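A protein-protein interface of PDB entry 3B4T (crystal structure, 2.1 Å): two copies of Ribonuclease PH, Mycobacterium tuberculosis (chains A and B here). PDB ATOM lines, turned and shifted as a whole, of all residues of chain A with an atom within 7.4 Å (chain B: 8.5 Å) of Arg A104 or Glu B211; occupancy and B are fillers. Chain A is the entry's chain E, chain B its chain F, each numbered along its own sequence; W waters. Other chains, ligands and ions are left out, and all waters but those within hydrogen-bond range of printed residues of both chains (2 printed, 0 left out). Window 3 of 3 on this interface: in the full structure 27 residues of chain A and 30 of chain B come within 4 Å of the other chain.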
ATOM      1  N   GLY A  62     -17.100  19.718   3.886  1.00  0.00           N
ATOM      2  CA  GLY A  62     -17.290  21.140   3.666  1.00  0.00           C
ATOM      3  C   GLY A  62     -16.908  21.975   4.873  1.00  0.00           C
ATOM      4  O   GLY A  62     -16.563  21.439   5.926  1.00  0.00           O
ATOM      5  N   TRP A  63     -16.969  23.293   4.719  1.00  0.00           N
ATOM      6  CA  TRP A  63     -16.640  24.202   5.810  1.00  0.00           C
ATOM      7  C   TRP A  63     -17.628  25.360   5.890  1.00  0.00           C
ATOM      8  O   TRP A  63     -18.213  25.764   4.886  1.00  0.00           O
ATOM      9  CB  TRP A  63     -15.211  24.734   5.655  1.00  0.00           C
ATOM     10  CG  TRP A  63     -14.758  25.592   6.798  1.00  0.00           C
ATOM     11  CD1 TRP A  63     -14.370  26.900   6.740  1.00  0.00           C
ATOM     12  CD2 TRP A  63     -14.651  25.206   8.174  1.00  0.00           C
ATOM     13  NE1 TRP A  63     -14.024  27.350   7.992  1.00  0.00           N
ATOM     14  CE2 TRP A  63     -14.189  26.326   8.891  1.00  0.00           C
ATOM     15  CE3 TRP A  63     -14.899  24.016   8.869  1.00  0.00           C
ATOM     16  CZ2 TRP A  63     -13.971  26.296  10.267  1.00  0.00           C
ATOM     17  CZ3 TRP A  63     -14.682  23.987  10.234  1.00  0.00           C
ATOM     18  CH2 TRP A  63     -14.223  25.119  10.919  1.00  0.00           C
ATOM     19  N   LEU A  64     -17.815  25.885   7.097  1.00  0.00           N
ATOM     20  CA  LEU A  64     -18.669  27.045   7.306  1.00  0.00           C
ATOM     21  C   LEU A  64     -17.926  28.098   8.117  1.00  0.00           C
ATOM     22  O   LEU A  64     -17.272  27.784   9.109  1.00  0.00           O
ATOM     23  CB  LEU A  64     -19.966  26.643   8.014  1.00  0.00           C
ATOM     24  CG  LEU A  64     -20.988  27.743   8.328  1.00  0.00           C
ATOM     25  CD1 LEU A  64     -22.382  27.152   8.464  1.00  0.00           C
ATOM     26  CD2 LEU A  64     -20.611  28.520   9.585  1.00  0.00           C
ATOM     27  N   THR A  65     -18.022  29.348   7.684  1.00  0.00           N
ATOM     28  CA  THR A  65     -17.453  30.452   8.442  1.00  0.00           C
ATOM     29  C   THR A  65     -18.528  31.506   8.681  1.00  0.00           C
ATOM     30  O   THR A  65     -19.491  31.589   7.925  1.00  0.00           O
ATOM     31  CB  THR A  65     -16.255  31.090   7.713  1.00  0.00           C
ATOM     32  OG1 THR A  65     -15.609  32.027   8.585  1.00  0.00           O
ATOM     33  CG2 THR A  65     -16.714  31.805   6.450  1.00  0.00           C
ATOM     34  N   ALA A  66     -18.363  32.308   9.726  1.00  0.00           N
ATOM     35  CA  ALA A  66     -19.366  33.298  10.086  1.00  0.00           C
ATOM     36  C   ALA A  66     -18.744  34.629  10.432  1.00  0.00           C
ATOM     37  O   ALA A  66     -17.696  34.688  11.094  1.00  0.00           O
ATOM     38  CB  ALA A  66     -20.211  32.796  11.236  1.00  0.00           C
ATOM     39  N   SER A  96     -18.404  36.730  16.021  1.00  0.00           N
ATOM     40  CA  SER A  96     -18.241  36.024  14.748  1.00  0.00           C
ATOM     41  C   SER A  96     -17.868  34.558  14.956  1.00  0.00           C
ATOM     42  O   SER A  96     -18.421  33.669  14.308  1.00  0.00           O
ATOM     43  CB  SER A  96     -17.187  36.710  13.873  1.00  0.00           C
ATOM     44  OG  SER A  96     -17.580  38.026  13.528  1.00  0.00           O
ATOM     45  N   ARG A  97     -16.925  34.312  15.860  1.00  0.00           N
ATOM     46  CA  ARG A  97     -16.499  32.949  16.164  1.00  0.00           C
ATOM     47  C   ARG A  97     -17.640  32.136  16.769  1.00  0.00           C
ATOM     48  O   ARG A  97     -17.881  30.997  16.368  1.00  0.00           O
ATOM     49  CB  ARG A  97     -15.290  32.961  17.103  1.00  0.00           C
ATOM     50  CG  ARG A  97     -14.032  33.535  16.465  1.00  0.00           C
ATOM     51  CD  ARG A  97     -12.960  33.833  17.497  1.00  0.00           C
ATOM     52  NE  ARG A  97     -12.590  32.650  18.269  1.00  0.00           N
ATOM     53  CZ  ARG A  97     -11.712  31.737  17.863  1.00  0.00           C
ATOM     54  NH1 ARG A  97     -11.111  31.867  16.687  1.00  0.00           N
ATOM     55  NH2 ARG A  97     -11.435  30.693  18.633  1.00  0.00           N
ATOM     56  N   LEU A  98     -18.343  32.726  17.731  1.00  0.00           N
ATOM     57  CA  LEU A  98     -19.474  32.061  18.371  1.00  0.00           C
ATOM     58  C   LEU A  98     -20.530  31.626  17.354  1.00  0.00           C
ATOM     59  O   LEU A  98     -21.045  30.509  17.425  1.00  0.00           O
ATOM     60  CB  LEU A  98     -20.109  32.969  19.424  1.00  0.00           C
ATOM     61  CG  LEU A  98     -21.415  32.455  20.039  1.00  0.00           C
ATOM     62  CD1 LEU A  98     -21.179  31.177  20.831  1.00  0.00           C
ATOM     63  CD2 LEU A  98     -22.063  33.519  20.914  1.00  0.00           C
ATOM     64  N   ILE A  99     -20.853  32.506  16.411  1.00  0.00           N
ATOM     65  CA  ILE A  99     -21.855  32.191  15.398  1.00  0.00           C
ATOM     66  C   ILE A  99     -21.412  31.007  14.551  1.00  0.00           C
ATOM     67  O   ILE A  99     -22.185  30.083  14.301  1.00  0.00           O
ATOM     68  CB  ILE A  99     -22.137  33.393  14.474  1.00  0.00           C
ATOM     69  CG1 ILE A  99     -22.673  34.579  15.280  1.00  0.00           C
ATOM     70  CG2 ILE A  99     -23.124  33.005  13.378  1.00  0.00           C
ATOM     71  CD1 ILE A  99     -22.901  35.828  14.445  1.00  0.00           C
ATOM     72  N   GLY A 100     -20.159  31.039  14.111  1.00  0.00           N
ATOM     73  CA  GLY A 100     -19.609  29.972  13.297  1.00  0.00           C
ATOM     74  C   GLY A 100     -19.643  28.629  13.996  1.00  0.00           C
ATOM     75  O   GLY A 100     -20.082  27.634  13.421  1.00  0.00           O
ATOM     76  N   ARG A 101     -19.182  28.596  15.242  1.00  0.00           N
ATOM     77  CA  ARG A 101     -19.137  27.350  15.997  1.00  0.00           C
ATOM     78  C   ARG A 101     -20.541  26.800  16.235  1.00  0.00           C
ATOM     79  O   ARG A 101     -20.803  25.622  15.997  1.00  0.00           O
ATOM     80  CB  ARG A 101     -18.416  27.547  17.332  1.00  0.00           C
ATOM     81  CG  ARG A 101     -17.497  26.394  17.694  1.00  0.00           C
ATOM     82  CD  ARG A 101     -17.062  26.430  19.150  1.00  0.00           C
ATOM     83  NE  ARG A 101     -16.914  27.786  19.669  1.00  0.00           N
ATOM     84  CZ  ARG A 101     -17.686  28.303  20.618  1.00  0.00           C
ATOM     85  NH1 ARG A 101     -18.658  27.574  21.152  1.00  0.00           N
ATOM     86  NH2 ARG A 101     -17.487  29.543  21.040  1.00  0.00           N
ATOM     87  N   SER A 102     -21.438  27.665  16.705  1.00  0.00           N
ATOM     88  CA  SER A 102     -22.815  27.275  16.993  1.00  0.00           C
ATOM     89  C   SER A 102     -23.454  26.547  15.820  1.00  0.00           C
ATOM     90  O   SER A 102     -24.013  25.464  15.980  1.00  0.00           O
ATOM     91  CB  SER A 102     -23.654  28.503  17.350  1.00  0.00           C
ATOM     92  OG  SER A 102     -23.128  29.169  18.482  1.00  0.00           O
ATOM     93  N   LEU A 103     -23.372  27.153  14.639  1.00  0.00           N
ATOM     94  CA  LEU A 103     -23.985  26.589  13.442  1.00  0.00           C
ATOM     95  C   LEU A 103     -23.345  25.263  13.039  1.00  0.00           C
ATOM     96  O   LEU A 103     -24.040  24.322  12.659  1.00  0.00           O
ATOM     97  CB  LEU A 103     -23.923  27.589  12.283  1.00  0.00           C
ATOM     98  CG  LEU A 103     -24.815  28.823  12.432  1.00  0.00           C
ATOM     99  CD1 LEU A 103     -24.638  29.770  11.257  1.00  0.00           C
ATOM    100  CD2 LEU A 103     -26.269  28.405  12.574  1.00  0.00           C
ATOM    101  N   ARG A 104     -22.022  25.187  13.134  1.00  0.00           N
ATOM    102  CA  ARG A 104     -21.302  23.971  12.771  1.00  0.00           C
ATOM    103  C   ARG A 104     -21.640  22.811  13.706  1.00  0.00           C
ATOM    104  O   ARG A 104     -21.371  21.653  13.391  1.00  0.00           O
ATOM    105  CB  ARG A 104     -19.790  24.218  12.758  1.00  0.00           C
ATOM    106  CG  ARG A 104     -19.320  25.167  11.665  1.00  0.00           C
ATOM    107  CD  ARG A 104     -17.806  25.153  11.529  1.00  0.00           C
ATOM    108  NE  ARG A 104     -17.142  25.635  12.735  1.00  0.00           N
ATOM    109  CZ  ARG A 104     -16.657  26.864  12.882  1.00  0.00           C
ATOM    110  NH1 ARG A 104     -16.069  27.213  14.016  1.00  0.00           N
ATOM    111  NH2 ARG A 104     -16.759  27.746  11.896  1.00  0.00           N
ATOM    112  N   ALA A 105     -22.232  23.129  14.854  1.00  0.00           N
ATOM    113  CA  ALA A 105     -22.593  22.112  15.838  1.00  0.00           C
ATOM    114  C   ALA A 105     -23.822  21.315  15.408  1.00  0.00           C
ATOM    115  O   ALA A 105     -24.080  20.232  15.928  1.00  0.00           O
ATOM    116  CB  ALA A 105     -22.823  22.748  17.201  1.00  0.00           C
ATOM    117  N   CYS A 106     -24.579  21.854  14.459  1.00  0.00           N
ATOM    118  CA  CYS A 106     -25.774  21.174  13.969  1.00  0.00           C
ATOM    119  C   CYS A 106     -25.700  20.869  12.475  1.00  0.00           C
ATOM    120  O   CYS A 106     -26.724  20.703  11.814  1.00  0.00           O
ATOM    121  CB  CYS A 106     -27.032  21.986  14.293  1.00  0.00           C
ATOM    122  SG  CYS A 106     -27.541  21.896  16.030  1.00  0.00           S
ATOM    123  N   ILE A 107     -24.480  20.797  11.949  1.00  0.00           N
ATOM    124  CA  ILE A 107     -24.266  20.383  10.567  1.00  0.00           C
ATOM    125  C   ILE A 107     -23.261  19.243  10.502  1.00  0.00           C
ATOM    126  O   ILE A 107     -22.251  19.252  11.208  1.00  0.00           O
ATOM    127  CB  ILE A 107     -23.712  21.525   9.693  1.00  0.00           C
ATOM    128  CG1 ILE A 107     -24.478  22.825   9.926  1.00  0.00           C
ATOM    129  CG2 ILE A 107     -23.755  21.136   8.221  1.00  0.00           C
ATOM    130  CD1 ILE A 107     -23.834  24.017   9.252  1.00  0.00           C
ATOM    131  N   ASP A 108     -23.543  18.260   9.654  1.00  0.00           N
ATOM    132  CA  ASP A 108     -22.570  17.226   9.341  1.00  0.00           C
ATOM    133  C   ASP A 108     -21.861  17.630   8.056  1.00  0.00           C
ATOM    134  O   ASP A 108     -22.358  17.388   6.958  1.00  0.00           O
ATOM    135  CB  ASP A 108     -23.251  15.866   9.178  1.00  0.00           C
ATOM    136  CG  ASP A 108     -22.266  14.711   9.210  1.00  0.00           C
ATOM    137  OD1 ASP A 108     -21.164  14.847   8.636  1.00  0.00           O
ATOM    138  OD2 ASP A 108     -22.596  13.664   9.807  1.00  0.00           O
ATOM    139  N   LEU A 109     -20.704  18.267   8.205  1.00  0.00           N
ATOM    140  CA  LEU A 109     -19.965  18.804   7.069  1.00  0.00           C
ATOM    141  C   LEU A 109     -19.677  17.743   6.007  1.00  0.00           C
ATOM    142  O   LEU A 109     -19.572  18.055   4.821  1.00  0.00           O
ATOM    143  CB  LEU A 109     -18.666  19.458   7.545  1.00  0.00           C
ATOM    144  CG  LEU A 109     -18.846  20.618   8.528  1.00  0.00           C
ATOM    145  CD1 LEU A 109     -17.507  21.075   9.089  1.00  0.00           C
ATOM    146  CD2 LEU A 109     -19.577  21.777   7.864  1.00  0.00           C
ATOM    147  N   LEU A 142     -29.001  29.369   6.841  1.00  0.00           N
ATOM    148  CA  LEU A 142     -28.236  28.153   6.604  1.00  0.00           C
ATOM    149  C   LEU A 142     -29.121  27.046   6.036  1.00  0.00           C
ATOM    150  O   LEU A 142     -28.713  26.316   5.135  1.00  0.00           O
ATOM    151  CB  LEU A 142     -27.585  27.680   7.904  1.00  0.00           C
ATOM    152  CG  LEU A 142     -27.055  26.248   7.931  1.00  0.00           C
ATOM    153  CD1 LEU A 142     -25.900  26.084   6.958  1.00  0.00           C
ATOM    154  CD2 LEU A 142     -26.632  25.877   9.340  1.00  0.00           C
ATOM    155  N   SER A 162     -28.447  18.234  11.371  1.00  0.00           N
ATOM    156  CA  SER A 162     -28.759  17.249  12.402  1.00  0.00           C
ATOM    157  C   SER A 162     -29.602  17.833  13.532  1.00  0.00           C
ATOM    158  O   SER A 162     -30.136  17.098  14.362  1.00  0.00           O
ATOM    159  CB  SER A 162     -27.472  16.650  12.968  1.00  0.00           C
ATOM    160  OG  SER A 162     -26.609  17.668  13.440  1.00  0.00           O
ATOM    161  N   ILE A 165     -30.620  25.404  15.562  1.00  0.00           N
ATOM    162  CA  ILE A 165     -29.926  26.264  16.511  1.00  0.00           C
ATOM    163  C   ILE A 165     -30.674  27.573  16.707  1.00  0.00           C
ATOM    164  O   ILE A 165     -31.083  28.214  15.743  1.00  0.00           O
ATOM    165  CB  ILE A 165     -28.496  26.591  16.035  1.00  0.00           C
ATOM    166  CG1 ILE A 165     -27.574  25.389  16.234  1.00  0.00           C
ATOM    167  CG2 ILE A 165     -27.946  27.789  16.789  1.00  0.00           C
ATOM    168  CD1 ILE A 165     -27.293  25.078  17.689  1.00  0.00           C
ATOM    169  N   ASP B 186      -7.578  17.266  25.191  1.00  0.00           N
ATOM    170  CA  ASP B 186      -8.399  18.351  24.668  1.00  0.00           C
ATOM    171  C   ASP B 186      -8.711  18.176  23.180  1.00  0.00           C
ATOM    172  O   ASP B 186      -9.692  18.723  22.674  1.00  0.00           O
ATOM    173  CB  ASP B 186      -7.704  19.693  24.916  1.00  0.00           C
ATOM    174  CG  ASP B 186      -8.524  20.873  24.447  1.00  0.00           C
ATOM    175  OD1 ASP B 186      -9.770  20.789  24.486  1.00  0.00           O
ATOM    176  OD2 ASP B 186      -7.922  21.890  24.046  1.00  0.00           O
ATOM    177  N   SER B 187      -7.881  17.407  22.486  1.00  0.00           N
ATOM    178  CA  SER B 187      -8.063  17.193  21.054  1.00  0.00           C
ATOM    179  C   SER B 187      -9.039  16.055  20.753  1.00  0.00           C
ATOM    180  O   SER B 187      -9.456  15.876  19.609  1.00  0.00           O
ATOM    181  CB  SER B 187      -6.717  16.934  20.373  1.00  0.00           C
ATOM    182  OG  SER B 187      -6.063  15.811  20.939  1.00  0.00           O
ATOM    183  N   ALA B 189     -11.643  15.509  23.151  1.00  0.00           N
ATOM    184  CA  ALA B 189     -12.757  15.791  24.048  1.00  0.00           C
ATOM    185  C   ALA B 189     -14.099  15.803  23.324  1.00  0.00           C
ATOM    186  O   ALA B 189     -14.262  16.477  22.307  1.00  0.00           O
ATOM    187  CB  ALA B 189     -12.534  17.109  24.774  1.00  0.00           C
ATOM    188  N   GLU B 190     -15.052  15.048  23.858  1.00  0.00           N
ATOM    189  CA  GLU B 190     -16.414  15.050  23.341  1.00  0.00           C
ATOM    190  C   GLU B 190     -17.024  16.436  23.529  1.00  0.00           C
ATOM    191  O   GLU B 190     -17.769  16.920  22.682  1.00  0.00           O
ATOM    192  CB  GLU B 190     -17.256  13.992  24.055  1.00  0.00           C
ATOM    193  CG  GLU B 190     -18.699  13.915  23.580  1.00  0.00           C
ATOM    194  CD  GLU B 190     -19.544  12.982  24.426  1.00  0.00           C
ATOM    195  OE1 GLU B 190     -20.750  13.263  24.596  1.00  0.00           O
ATOM    196  OE2 GLU B 190     -19.003  11.972  24.926  1.00  0.00           O
ATOM    197  N   VAL B 191     -16.695  17.068  24.650  1.00  0.00           N
ATOM    198  CA  VAL B 191     -17.141  18.426  24.931  1.00  0.00           C
ATOM    199  C   VAL B 191     -16.122  19.150  25.809  1.00  0.00           C
ATOM    200  O   VAL B 191     -15.584  18.576  26.754  1.00  0.00           O
ATOM    201  CB  VAL B 191     -18.530  18.446  25.604  1.00  0.00           C
ATOM    202  CG1 VAL B 191     -18.554  17.518  26.805  1.00  0.00           C
ATOM    203  CG2 VAL B 191     -18.904  19.861  26.010  1.00  0.00           C
ATOM    204  N   ASP B 192     -15.858  20.410  25.481  1.00  0.00           N
ATOM    205  CA  ASP B 192     -14.853  21.201  26.183  1.00  0.00           C
ATOM    206  C   ASP B 192     -15.456  22.474  26.742  1.00  0.00           C
ATOM    207  O   ASP B 192     -16.485  22.944  26.263  1.00  0.00           O
ATOM    208  CB  ASP B 192     -13.723  21.584  25.226  1.00  0.00           C
ATOM    209  CG  ASP B 192     -12.670  20.511  25.111  1.00  0.00           C
ATOM    210  OD1 ASP B 192     -12.344  20.119  23.971  1.00  0.00           O
ATOM    211  OD2 ASP B 192     -12.170  20.058  26.161  1.00  0.00           O
ATOM    212  N   MET B 193     -14.805  23.033  27.756  1.00  0.00           N
ATOM    213  CA  MET B 193     -15.130  24.380  28.209  1.00  0.00           C
ATOM    214  C   MET B 193     -14.261  24.850  29.368  1.00  0.00           C
ATOM    215  O   MET B 193     -13.522  24.071  29.972  1.00  0.00           O
ATOM    216  CB  MET B 193     -16.611  24.508  28.562  1.00  0.00           C
ATOM    217  CG  MET B 193     -17.053  23.681  29.747  1.00  0.00           C
ATOM    218  SD  MET B 193     -18.850  23.559  29.770  1.00  0.00           S
ATOM    219  CE  MET B 193     -19.134  22.542  28.326  1.00  0.00           C
ATOM    220  N   GLY B 208     -16.251  28.969  25.917  1.00  0.00           N
ATOM    221  CA  GLY B 208     -15.489  28.229  24.927  1.00  0.00           C
ATOM    222  C   GLY B 208     -15.745  26.738  24.872  1.00  0.00           C
ATOM    223  O   GLY B 208     -14.883  25.938  25.238  1.00  0.00           O
ATOM    224  N   THR B 209     -16.929  26.360  24.401  1.00  0.00           N
ATOM    225  CA  THR B 209     -17.246  24.954  24.192  1.00  0.00           C
ATOM    226  C   THR B 209     -16.440  24.422  23.010  1.00  0.00           C
ATOM    227  O   THR B 209     -16.236  25.128  22.022  1.00  0.00           O
ATOM    228  CB  THR B 209     -18.753  24.739  23.948  1.00  0.00           C
ATOM    229  OG1 THR B 209     -19.500  25.331  25.020  1.00  0.00           O
ATOM    230  CG2 THR B 209     -19.076  23.252  23.866  1.00  0.00           C
ATOM    231  N   GLY B 210     -15.970  23.184  23.124  1.00  0.00           N
ATOM    232  CA  GLY B 210     -15.150  22.578  22.090  1.00  0.00           C
ATOM    233  C   GLY B 210     -15.807  22.570  20.721  1.00  0.00           C
ATOM    234  O   GLY B 210     -17.031  22.477  20.607  1.00  0.00           O
ATOM    235  N   GLU B 211     -14.987  22.667  19.679  1.00  0.00           N
ATOM    236  CA  GLU B 211     -15.481  22.682  18.306  1.00  0.00           C
ATOM    237  C   GLU B 211     -16.433  21.520  18.025  1.00  0.00           C
ATOM    238  O   GLU B 211     -16.056  20.354  18.137  1.00  0.00           O
ATOM    239  CB  GLU B 211     -14.312  22.662  17.315  1.00  0.00           C
ATOM    240  CG  GLU B 211     -14.729  22.580  15.854  1.00  0.00           C
ATOM    241  CD  GLU B 211     -15.535  23.785  15.406  1.00  0.00           C
ATOM    242  OE1 GLU B 211     -16.363  23.636  14.483  1.00  0.00           O
ATOM    243  OE2 GLU B 211     -15.343  24.882  15.973  1.00  0.00           O
ATOM    244  N   GLY B 212     -17.670  21.852  17.666  1.00  0.00           N
ATOM    245  CA  GLY B 212     -18.655  20.858  17.277  1.00  0.00           C
ATOM    246  C   GLY B 212     -19.332  20.163  18.441  1.00  0.00           C
ATOM    247  O   GLY B 212     -20.103  19.222  18.247  1.00  0.00           O
ATOM    248  N   ALA B 213     -19.056  20.630  19.655  1.00  0.00           N
ATOM    249  CA  ALA B 213     -19.564  19.971  20.853  1.00  0.00           C
ATOM    250  C   ALA B 213     -20.836  20.610  21.405  1.00  0.00           C
ATOM    251  O   ALA B 213     -20.945  21.835  21.494  1.00  0.00           O
ATOM    252  CB  ALA B 213     -18.484  19.924  21.928  1.00  0.00           C
ATOM    253  N   THR B 214     -21.795  19.764  21.765  1.00  0.00           N
ATOM    254  CA  THR B 214     -22.977  20.187  22.505  1.00  0.00           C
ATOM    255  C   THR B 214     -23.096  19.334  23.765  1.00  0.00           C
ATOM    256  O   THR B 214     -22.493  18.262  23.852  1.00  0.00           O
ATOM    257  CB  THR B 214     -24.265  20.063  21.667  1.00  0.00           C
ATOM    258  OG1 THR B 214     -24.505  18.686  21.347  1.00  0.00           O
ATOM    259  CG2 THR B 214     -24.146  20.870  20.380  1.00  0.00           C
HETATM  260  O   HOH W   1     -14.077  26.668  20.692  1.00  0.00           O
HETATM  261  O   HOH W   2     -19.793  23.576  17.563  1.00  0.00           O
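The guanidinium group (NE) of Arg A104 lies within salt-bridge range of the side-chain carboxylate (OE1) of Glu B211 (2.8 Å).
NH2 of Arg A104 is in hydrogen-bond range of O of Leu A64 (2.8 Å).
Among the printed residues, merely in contact across the chains: Arg A101 with Glu B211, Arg A101 with Thr B209 and Ala A105 with Thr B214.
Printed residues of chain B within 4 Å of Arg A101: Thr B209 (3.3 Å) and Glu B211 (3.1 Å).
Leu A103 touches none of the printed residues of chain B.
Arg A104 touches one residue of chain B.
Of the printed residues of chain A, Thr B209 touches Arg A101 (3.3 Å).
Glu B211 touches just these residues of chain A: Arg A101 (3.1 Å) and Arg A104 (2.8 Å).
Of the printed residues of chain A, Thr B214 touches Ala A105 (3.9 Å).
The nearest residue of chain A that does not touch Glu B211 is Trp A63 (4.4 Å).
The nearest printed residue of chain B that does not touch Arg A101 is Gly B210 (4.2 Å).
Of the 22 printed residues of chain A, 3 touch a printed residue of chain B.
Printed residues of chain A that touch a printed residue of chain B: Arg A101, Arg A104 and Ala A105.
Hydrophobic or aromatic side chains of chain A that line the printed part of chain B: Ala A105.
No position is printed for both chains.
Water W2 lies within hydrogen-bond range of the backbone NH of Gly B212 and the backbone carbonyl oxygen of Arg A101.
Water W1 lies within hydrogen-bond range of the backbone carbonyl oxygen of Thr B209 (3.0 Å) and the guanidinium group of Arg A101 (3.2 Å).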
